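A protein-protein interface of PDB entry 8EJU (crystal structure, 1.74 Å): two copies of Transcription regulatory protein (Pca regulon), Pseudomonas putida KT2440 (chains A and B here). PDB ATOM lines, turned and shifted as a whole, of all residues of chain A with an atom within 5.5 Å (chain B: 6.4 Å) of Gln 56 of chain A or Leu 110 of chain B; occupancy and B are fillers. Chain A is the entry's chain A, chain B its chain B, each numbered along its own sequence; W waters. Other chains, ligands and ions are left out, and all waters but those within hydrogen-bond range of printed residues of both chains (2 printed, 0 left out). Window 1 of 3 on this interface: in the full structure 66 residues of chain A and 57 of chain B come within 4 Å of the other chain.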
ATOM      1  N   GLY A  51       4.335  17.703   7.074  1.00  0.00           N
ATOM      2  CA  GLY A  51       4.305  18.488   5.831  1.00  0.00           C
ATOM      3  C   GLY A  51       4.129  19.980   6.112  1.00  0.00           C
ATOM      4  O   GLY A  51       4.765  20.812   5.460  1.00  0.00           O
ATOM      5  N   LEU A  52       3.307  20.316   7.109  1.00  0.00           N
ATOM      6  CA  LEU A  52       3.165  21.732   7.486  1.00  0.00           C
ATOM      7  C   LEU A  52       4.480  22.266   8.018  1.00  0.00           C
ATOM      8  O   LEU A  52       4.875  23.399   7.686  1.00  0.00           O
ATOM      9  CB  LEU A  52       2.075  21.963   8.517  1.00  0.00           C
ATOM     10  CG  LEU A  52       0.731  21.594   7.896  1.00  0.00           C
ATOM     11  CD1 LEU A  52      -0.258  21.380   9.042  1.00  0.00           C
ATOM     12  CD2 LEU A  52       0.305  22.735   6.926  1.00  0.00           C
ATOM     13  N   ALA A  53       5.203  21.447   8.806  1.00  0.00           N
ATOM     14  CA  ALA A  53       6.499  21.877   9.305  1.00  0.00           C
ATOM     15  C   ALA A  53       7.518  22.029   8.155  1.00  0.00           C
ATOM     16  O   ALA A  53       8.448  22.862   8.240  1.00  0.00           O
ATOM     17  CB  ALA A  53       7.007  20.877  10.373  1.00  0.00           C
ATOM     18  N   VAL A  54       7.420  21.182   7.127  1.00  0.00           N
ATOM     19  CA  VAL A  54       8.319  21.295   5.983  1.00  0.00           C
ATOM     20  C   VAL A  54       8.057  22.599   5.252  1.00  0.00           C
ATOM     21  O   VAL A  54       9.004  23.303   4.871  1.00  0.00           O
ATOM     22  CB  VAL A  54       8.150  20.063   5.068  1.00  0.00           C
ATOM     23  CG1 VAL A  54       8.793  20.300   3.706  1.00  0.00           C
ATOM     24  CG2 VAL A  54       8.748  18.807   5.798  1.00  0.00           C
ATOM     25  N   ILE A  55       6.781  22.987   5.106  1.00  0.00           N
ATOM     26  CA  ILE A  55       6.507  24.316   4.497  1.00  0.00           C
ATOM     27  C   ILE A  55       7.120  25.416   5.347  1.00  0.00           C
ATOM     28  O   ILE A  55       7.774  26.347   4.838  1.00  0.00           O
ATOM     29  CB  ILE A  55       4.994  24.528   4.334  1.00  0.00           C
ATOM     30  CG1 ILE A  55       4.491  23.628   3.221  1.00  0.00           C
ATOM     31  CG2 ILE A  55       4.693  26.013   3.884  1.00  0.00           C
ATOM     32  CD1 ILE A  55       2.862  23.517   3.192  1.00  0.00           C
ATOM     33  N   GLN A  56       6.949  25.312   6.665  1.00  0.00           N
ATOM     34  CA  GLN A  56       7.435  26.375   7.564  1.00  0.00           C
ATOM     35  C   GLN A  56       8.949  26.457   7.503  1.00  0.00           C
ATOM     36  O   GLN A  56       9.526  27.493   7.842  1.00  0.00           O
ATOM     37  CB  GLN A  56       6.979  26.127   9.014  1.00  0.00           C
ATOM     38  CG  GLN A  56       5.446  26.208   9.210  1.00  0.00           C
ATOM     39  CD  GLN A  56       4.909  27.687   9.177  1.00  0.00           C
ATOM     40  OE1 GLN A  56       5.699  28.644   9.147  1.00  0.00           O
ATOM     41  NE2 GLN A  56       3.587  27.863   9.190  1.00  0.00           N
ATOM     42  N   ALA A  57       9.619  25.322   7.189  1.00  0.00           N
ATOM     43  CA  ALA A  57      11.070  25.315   7.174  1.00  0.00           C
ATOM     44  C   ALA A  57      11.613  26.341   6.172  1.00  0.00           C
ATOM     45  O   ALA A  57      12.776  26.747   6.297  1.00  0.00           O
ATOM     46  CB  ALA A  57      11.591  23.903   6.849  1.00  0.00           C
ATOM     47  N   PHE A  58      10.786  26.767   5.198  1.00  0.00           N
ATOM     48  CA  PHE A  58      11.256  27.724   4.183  1.00  0.00           C
ATOM     49  C   PHE A  58      11.271  29.154   4.692  1.00  0.00           C
ATOM     50  O   PHE A  58      11.790  30.030   3.998  1.00  0.00           O
ATOM     51  CB  PHE A  58      10.371  27.622   2.940  1.00  0.00           C
ATOM     52  CG  PHE A  58      10.708  26.432   2.100  1.00  0.00           C
ATOM     53  CD1 PHE A  58      10.185  25.187   2.381  1.00  0.00           C
ATOM     54  CD2 PHE A  58      11.612  26.573   1.064  1.00  0.00           C
ATOM     55  CE1 PHE A  58      10.528  24.099   1.564  1.00  0.00           C
ATOM     56  CE2 PHE A  58      11.962  25.529   0.288  1.00  0.00           C
ATOM     57  CZ  PHE A  58      11.425  24.268   0.522  1.00  0.00           C
ATOM     58  N   GLN A  59      10.740  29.413   5.888  1.00  0.00           N
ATOM     59  CA  GLN A  59      10.553  30.809   6.331  1.00  0.00           C
ATOM     60  C   GLN A  59      11.862  31.582   6.258  1.00  0.00           C
ATOM     61  O   GLN A  59      12.887  31.166   6.820  1.00  0.00           O
ATOM     62  CB  GLN A  59      10.034  30.872   7.771  1.00  0.00           C
ATOM     63  CG  GLN A  59       8.614  30.554   7.896  1.00  0.00           C
ATOM     64  CD  GLN A  59       7.623  31.621   7.445  1.00  0.00           C
ATOM     65  OE1 GLN A  59       7.922  32.611   6.722  1.00  0.00           O
ATOM     66  NE2 GLN A  59       6.377  31.328   7.758  1.00  0.00           N
ATOM     67  N   ARG A  73      16.744  21.642  10.099  1.00  0.00           N
ATOM     68  CA  ARG A  73      16.030  22.748  10.736  1.00  0.00           C
ATOM     69  C   ARG A  73      14.803  22.249  11.498  1.00  0.00           C
ATOM     70  O   ARG A  73      14.488  22.770  12.575  1.00  0.00           O
ATOM     71  CB  ARG A  73      15.656  23.800   9.674  1.00  0.00           C
ATOM     72  CG  ARG A  73      14.626  24.852  10.124  1.00  0.00           C
ATOM     73  CD  ARG A  73      14.606  26.149   9.236  1.00  0.00           C
ATOM     74  NE  ARG A  73      14.356  27.370  10.004  1.00  0.00           N
ATOM     75  CZ  ARG A  73      13.739  28.460   9.547  1.00  0.00           C
ATOM     76  NH1 ARG A  73      13.380  28.582   8.273  1.00  0.00           N
ATOM     77  NH2 ARG A  73      13.492  29.464  10.385  1.00  0.00           N
ATOM     78  N   LEU A 103       9.194  26.231  -2.694  1.00  0.00           N
ATOM     79  CA  LEU A 103       7.748  26.235  -2.680  1.00  0.00           C
ATOM     80  C   LEU A 103       7.182  26.937  -3.939  1.00  0.00           C
ATOM     81  O   LEU A 103       7.843  27.751  -4.604  1.00  0.00           O
ATOM     82  CB  LEU A 103       7.225  26.980  -1.441  1.00  0.00           C
ATOM     83  CG  LEU A 103       7.622  26.349  -0.092  1.00  0.00           C
ATOM     84  CD1 LEU A 103       7.237  27.295   1.069  1.00  0.00           C
ATOM     85  CD2 LEU A 103       6.891  25.007   0.053  1.00  0.00           C
ATOM     86  N   VAL A 107       1.005  27.747  -2.446  1.00  0.00           N
ATOM     87  CA  VAL A 107       1.027  27.876  -0.990  1.00  0.00           C
ATOM     88  C   VAL A 107       0.265  29.113  -0.521  1.00  0.00           C
ATOM     89  O   VAL A 107      -0.342  29.132   0.559  1.00  0.00           O
ATOM     90  CB  VAL A 107       2.493  27.894  -0.512  1.00  0.00           C
ATOM     91  CG1 VAL A 107       2.562  28.173   0.946  1.00  0.00           C
ATOM     92  CG2 VAL A 107       3.133  26.500  -0.800  1.00  0.00           C
ATOM     93  N   LEU A 110      -3.342  28.893   0.528  1.00  0.00           N
ATOM     94  CA  LEU A 110      -3.693  28.468   1.885  1.00  0.00           C
ATOM     95  C   LEU A 110      -3.977  29.679   2.772  1.00  0.00           C
ATOM     96  O   LEU A 110      -4.973  29.731   3.485  1.00  0.00           O
ATOM     97  CB  LEU A 110      -2.568  27.613   2.460  1.00  0.00           C
ATOM     98  CG  LEU A 110      -2.361  26.309   1.649  1.00  0.00           C
ATOM     99  CD1 LEU A 110      -1.022  25.657   2.038  1.00  0.00           C
ATOM    100  CD2 LEU A 110      -3.493  25.249   1.936  1.00  0.00           C
ATOM    101  N   ARG A 171       5.474  38.392  10.969  1.00  0.00           N
ATOM    102  CA  ARG A 171       5.425  38.395  12.431  1.00  0.00           C
ATOM    103  C   ARG A 171       6.472  39.353  13.028  1.00  0.00           C
ATOM    104  O   ARG A 171       7.577  39.508  12.487  1.00  0.00           O
ATOM    105  CB  ARG A 171       5.668  36.956  12.926  1.00  0.00           C
ATOM    106  CG  ARG A 171       4.377  36.188  13.008  1.00  0.00           C
ATOM    107  CD  ARG A 171       4.596  34.724  13.225  1.00  0.00           C
ATOM    108  NE  ARG A 171       5.311  34.070  12.133  1.00  0.00           N
ATOM    109  CZ  ARG A 171       5.781  32.834  12.201  1.00  0.00           C
ATOM    110  NH1 ARG A 171       5.802  32.175  13.349  1.00  0.00           N
ATOM    111  NH2 ARG A 171       6.251  32.251  11.094  1.00  0.00           N
ATOM    112  N   LEU B  52      -4.214  19.654   3.624  1.00  0.00           N
ATOM    113  CA  LEU B  52      -4.154  20.887   2.807  1.00  0.00           C
ATOM    114  C   LEU B  52      -5.477  21.114   2.061  1.00  0.00           C
ATOM    115  O   LEU B  52      -5.930  22.255   1.935  1.00  0.00           O
ATOM    116  CB  LEU B  52      -3.015  20.777   1.805  1.00  0.00           C
ATOM    117  CG  LEU B  52      -1.653  20.600   2.529  1.00  0.00           C
ATOM    118  CD1 LEU B  52      -0.598  20.312   1.464  1.00  0.00           C
ATOM    119  CD2 LEU B  52      -1.311  21.867   3.310  1.00  0.00           C
ATOM    120  N   ILE B  55      -7.908  22.744   4.421  1.00  0.00           N
ATOM    121  CA  ILE B  55      -7.690  24.178   4.535  1.00  0.00           C
ATOM    122  C   ILE B  55      -8.315  24.875   3.335  1.00  0.00           C
ATOM    123  O   ILE B  55      -9.017  25.884   3.473  1.00  0.00           O
ATOM    124  CB  ILE B  55      -6.190  24.519   4.629  1.00  0.00           C
ATOM    125  CG1 ILE B  55      -5.558  24.054   5.954  1.00  0.00           C
ATOM    126  CG2 ILE B  55      -5.996  26.104   4.523  1.00  0.00           C
ATOM    127  CD1 ILE B  55      -4.045  24.226   6.022  1.00  0.00           C
ATOM    128  N   TYR B  93      -3.583  25.919  13.623  1.00  0.00           N
ATOM    129  CA  TYR B  93      -4.035  26.418  12.326  1.00  0.00           C
ATOM    130  C   TYR B  93      -5.533  26.560  12.261  1.00  0.00           C
ATOM    131  O   TYR B  93      -6.047  27.115  11.303  1.00  0.00           O
ATOM    132  CB  TYR B  93      -3.573  25.464  11.218  1.00  0.00           C
ATOM    133  CG  TYR B  93      -2.090  25.531  10.958  1.00  0.00           C
ATOM    134  CD1 TYR B  93      -1.539  26.553  10.194  1.00  0.00           C
ATOM    135  CD2 TYR B  93      -1.249  24.566  11.475  1.00  0.00           C
ATOM    136  CE1 TYR B  93      -0.175  26.608   9.984  1.00  0.00           C
ATOM    137  CE2 TYR B  93       0.121  24.603  11.273  1.00  0.00           C
ATOM    138  CZ  TYR B  93       0.644  25.630  10.498  1.00  0.00           C
ATOM    139  OH  TYR B  93       1.987  25.700  10.274  1.00  0.00           O
ATOM    140  N   LYS B 106      -2.730  31.760  11.774  1.00  0.00           N
ATOM    141  CA  LYS B 106      -1.462  31.082  11.525  1.00  0.00           C
ATOM    142  C   LYS B 106      -1.377  30.522  10.108  1.00  0.00           C
ATOM    143  O   LYS B 106      -0.272  30.336   9.585  1.00  0.00           O
ATOM    144  CB  LYS B 106      -1.261  29.965  12.568  1.00  0.00           C
ATOM    145  CG  LYS B 106       0.124  29.237  12.524  1.00  0.00           C
ATOM    146  CD  LYS B 106       0.247  28.213  13.620  1.00  0.00           C
ATOM    147  CE  LYS B 106       1.660  27.541  13.632  1.00  0.00           C
ATOM    148  NZ  LYS B 106       1.743  26.647  14.781  1.00  0.00           N
ATOM    149  N   VAL B 107      -2.513  30.249   9.480  1.00  0.00           N
ATOM    150  CA  VAL B 107      -2.477  29.791   8.103  1.00  0.00           C
ATOM    151  C   VAL B 107      -1.747  30.802   7.224  1.00  0.00           C
ATOM    152  O   VAL B 107      -1.089  30.432   6.248  1.00  0.00           O
ATOM    153  CB  VAL B 107      -3.918  29.526   7.618  1.00  0.00           C
ATOM    154  CG1 VAL B 107      -3.938  29.288   6.208  1.00  0.00           C
ATOM    155  CG2 VAL B 107      -4.478  28.254   8.343  1.00  0.00           C
ATOM    156  N   LEU B 108      -1.824  32.090   7.556  1.00  0.00           N
ATOM    157  CA  LEU B 108      -1.158  33.080   6.715  1.00  0.00           C
ATOM    158  C   LEU B 108       0.341  32.900   6.719  1.00  0.00           C
ATOM    159  O   LEU B 108       1.011  33.363   5.799  1.00  0.00           O
ATOM    160  CB  LEU B 108      -1.433  34.521   7.204  1.00  0.00           C
ATOM    161  CG  LEU B 108      -2.900  34.926   7.137  1.00  0.00           C
ATOM    162  CD1 LEU B 108      -3.062  36.171   8.027  1.00  0.00           C
ATOM    163  CD2 LEU B 108      -3.371  35.188   5.702  1.00  0.00           C
ATOM    164  N   THR B 109       0.882  32.294   7.767  1.00  0.00           N
ATOM    165  CA  THR B 109       2.320  32.136   7.804  1.00  0.00           C
ATOM    166  C   THR B 109       2.781  31.083   6.802  1.00  0.00           C
ATOM    167  O   THR B 109       3.955  31.100   6.443  1.00  0.00           O
ATOM    168  CB  THR B 109       2.839  31.779   9.210  1.00  0.00           C
ATOM    169  OG1 THR B 109       2.366  30.490   9.655  1.00  0.00           O
ATOM    170  CG2 THR B 109       2.365  32.815  10.207  1.00  0.00           C
ATOM    171  N   LEU B 110       1.878  30.209   6.336  1.00  0.00           N
ATOM    172  CA  LEU B 110       2.289  29.281   5.261  1.00  0.00           C
ATOM    173  C   LEU B 110       2.575  30.053   3.991  1.00  0.00           C
ATOM    174  O   LEU B 110       3.618  29.900   3.352  1.00  0.00           O
ATOM    175  CB  LEU B 110       1.186  28.241   5.018  1.00  0.00           C
ATOM    176  CG  LEU B 110       0.903  27.377   6.239  1.00  0.00           C
ATOM    177  CD1 LEU B 110      -0.433  26.643   6.025  1.00  0.00           C
ATOM    178  CD2 LEU B 110       2.079  26.316   6.448  1.00  0.00           C
ATOM    179  N   GLY B 111       1.699  31.008   3.664  1.00  0.00           N
ATOM    180  CA  GLY B 111       1.983  31.777   2.469  1.00  0.00           C
ATOM    181  C   GLY B 111       3.231  32.626   2.641  1.00  0.00           C
ATOM    182  O   GLY B 111       3.940  32.921   1.671  1.00  0.00           O
ATOM    183  N   HIS B 112       3.453  33.150   3.871  1.00  0.00           N
ATOM    184  CA  HIS B 112       4.640  33.938   4.108  1.00  0.00           C
ATOM    185  C   HIS B 112       5.909  33.105   3.916  1.00  0.00           C
ATOM    186  O   HIS B 112       6.942  33.652   3.527  1.00  0.00           O
ATOM    187  CB  HIS B 112       4.592  34.531   5.512  1.00  0.00           C
ATOM    188  CG  HIS B 112       5.653  35.550   5.770  1.00  0.00           C
ATOM    189  ND1 HIS B 112       6.909  35.238   6.241  1.00  0.00           N
ATOM    190  CD2 HIS B 112       5.641  36.889   5.590  1.00  0.00           C
ATOM    191  CE1 HIS B 112       7.619  36.344   6.380  1.00  0.00           C
ATOM    192  NE2 HIS B 112       6.877  37.363   5.976  1.00  0.00           N
ATOM    193  N   ALA B 113       5.839  31.781   4.164  1.00  0.00           N
ATOM    194  CA  ALA B 113       6.983  30.907   3.878  1.00  0.00           C
ATOM    195  C   ALA B 113       7.338  30.941   2.395  1.00  0.00           C
ATOM    196  O   ALA B 113       8.524  30.974   2.037  1.00  0.00           O
ATOM    197  CB  ALA B 113       6.683  29.456   4.294  1.00  0.00           C
ATOM    198  N   TYR B 114       6.332  30.943   1.516  1.00  0.00           N
ATOM    199  CA  TYR B 114       6.595  31.068   0.081  1.00  0.00           C
ATOM    200  C   TYR B 114       7.172  32.444  -0.235  1.00  0.00           C
ATOM    201  O   TYR B 114       8.220  32.545  -0.897  1.00  0.00           O
ATOM    202  CB  TYR B 114       5.300  30.816  -0.716  1.00  0.00           C
ATOM    203  CG  TYR B 114       5.430  31.261  -2.134  1.00  0.00           C
ATOM    204  CD1 TYR B 114       6.084  30.450  -3.083  1.00  0.00           C
ATOM    205  CD2 TYR B 114       4.971  32.525  -2.549  1.00  0.00           C
ATOM    206  CE1 TYR B 114       6.288  30.858  -4.378  1.00  0.00           C
ATOM    207  CE2 TYR B 114       5.177  32.926  -3.845  1.00  0.00           C
ATOM    208  CZ  TYR B 114       5.805  32.118  -4.743  1.00  0.00           C
ATOM    209  OH  TYR B 114       5.982  32.607  -5.980  1.00  0.00           O
ATOM    210  N   LEU B 115       6.503  33.512   0.247  1.00  0.00           N
ATOM    211  CA  LEU B 115       6.937  34.856  -0.146  1.00  0.00           C
ATOM    212  C   LEU B 115       8.367  35.125   0.299  1.00  0.00           C
ATOM    213  O   LEU B 115       9.117  35.853  -0.373  1.00  0.00           O
ATOM    214  CB  LEU B 115       6.007  35.936   0.462  1.00  0.00           C
ATOM    215  CG  LEU B 115       4.585  35.845  -0.076  1.00  0.00           C
ATOM    216  CD1 LEU B 115       3.672  36.734   0.720  1.00  0.00           C
ATOM    217  CD2 LEU B 115       4.477  36.184  -1.578  1.00  0.00           C
HETATM  218  O   HOH W   1       5.597  34.584   9.291  1.00  0.00           O
HETATM  219  O   HOH W   2       3.800  29.946  12.131  1.00  0.00           O
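Ile 55 of chain A touches Leu 110 of chain B, and with the chains exchanged Leu 110 of chain A touches Ile 55 of chain B.
Val 107 of chain A touches Leu 110 of chain B, and with the chains exchanged Leu 110 of chain A touches Val 107 of chain B.
Leu 110 of chain A touches Leu 52 of chain B, but with the chains exchanged Leu 52 of chain A does not touch Leu 110 of chain B (4.02 Å).
Positions printed for both chains: 52, 55, 107 and 110.
Among the printed residues, pairs that only touch across the chains: Leu 52 of chain A with Tyr 93 of chain B (3.9 Å), Ile 55 of chain A with Leu 110 of chain B (3.7 Å), Ile 55 of chain A with Ala 113 of chain B (3.3 Å), Gln 56 of chain A with Leu 110 of chain B (3.5 Å), Phe 58 of chain A with Ala 113 of chain B (3.9 Å), Leu 103 of chain A with Ala 113 of chain B (3.9 Å), Leu 103 of chain A with Tyr 114 of chain B (3.5 Å), Val 107 of chain A with Leu 110 of chain B (3.1 Å), Val 107 of chain A with Gly 111 of chain B (3.96 Å), Leu 110 of chain A with Leu 52 of chain B (3.9 Å), Leu 110 of chain A with Ile 55 of chain B (3.7 Å), Leu 110 of chain A with Val 107 of chain B (2.9 Å) and Arg 171 of chain A with Thr 109 of chain B (3.7 Å).
Hydrophobic or aromatic side chains of chain A within 4 Å of the printed part of chain B: Leu 52, Ile 55, Phe 58, Leu 103, Val 107 and Leu 110.
Along chain A the printed residues that touch a printed residue of chain B span positions 52 to 171.
Printed residues of chain B that touch a printed residue of chain A: Leu 52, Ile 55, Tyr 93, Val 107, Thr 109, Leu 110, Gly 111, His 112, Ala 113 and Tyr 114.
Along chain B the printed residues that touch a printed residue of chain A span positions 52 to 114.
Among the printed residues, 18 pairs touch across the chains.
Among the printed residues, no Asp or Glu carboxylate lies within 4 Å of a Lys or Arg side-chain nitrogen of the other chain.
NE2 of Gln 56 of chain A lies within hydrogen-bond range of OH of Tyr 93 of chain B, 2.9 Å away.
The side-chain amide nitrogen of Gln 56 of chain A is in hydrogen-bond range of the side-chain hydroxyl of Thr 109 of chain B, 2.9 Å away.
The backbone carbonyl oxygen (O) of Thr 109 of chain B sits at hydrogen-bond distance from the side-chain amide nitrogen (NE2) of Gln 59 of chain A, at 2.8 Å.
A ring nitrogen (ND1) of His 112 of chain B lies within hydrogen-bond range of the side-chain amide oxygen (OE1) of Gln 59 of chain A (2.9 Å).
The side-chain amide oxygen (OE1) of Gln 59 of chain A is in hydrogen-bond range of the backbone NH (N) of Ala 113 of chain B (3.4 Å).
Of chain B, only Tyr 93 (2.9 Å), Thr 109 (2.9 Å) and Leu 110 (3.5 Å) come within 4 Å of Gln 56 of chain A.
Printed residues of chain A within 4 Å of Tyr 114 of chain B: Leu 103.
Of the printed residues of chain B, Val 107 of chain A touches Leu 110 and Gly 111.
Of the printed residues of chain A, Thr 109 of chain B touches Gln 56 (2.9 Å), Gln 59 (2.8 Å) and Arg 171 (3.7 Å).
Printed residues of chain A within 4 Å of Val 107 of chain B: Leu 110.
Leu 108 of chain B touches none of the printed residues of chain A.
Arg 73 of chain A touches none of the printed residues of chain B.
Water W1 bridges NE of Arg 171 of chain A (2.9 Å) and ND1 of His 112 of chain B (3.4 Å).
Water W2 lies within hydrogen-bond range of the side-chain hydroxyl of Thr 109 of chain B and the guanidinium group of Arg 171 of chain A.
The side-chain amide oxygen (OE1) of Gln 56 of chain A is in hydrogen-bond range of the side-chain amide nitrogen (NE2) of Gln 59 of chain A, 3.1 Å away.
The guanidinium group of Arg 73 of chain A is in hydrogen-bond range of the backbone carbonyl oxygen of Gln 59 of chain A (3.0 Å).
The side-chain amide nitrogen (NE2) of Gln 59 of chain A sits close to the guanidinium group (NH2) of Arg 171 of chain A (3.5 Å).
The backbone carbonyl oxygen (O) of Lys 106 of chain B lies within hydrogen-bond range of the side-chain hydroxyl (OG1) of Thr 109 of chain B.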
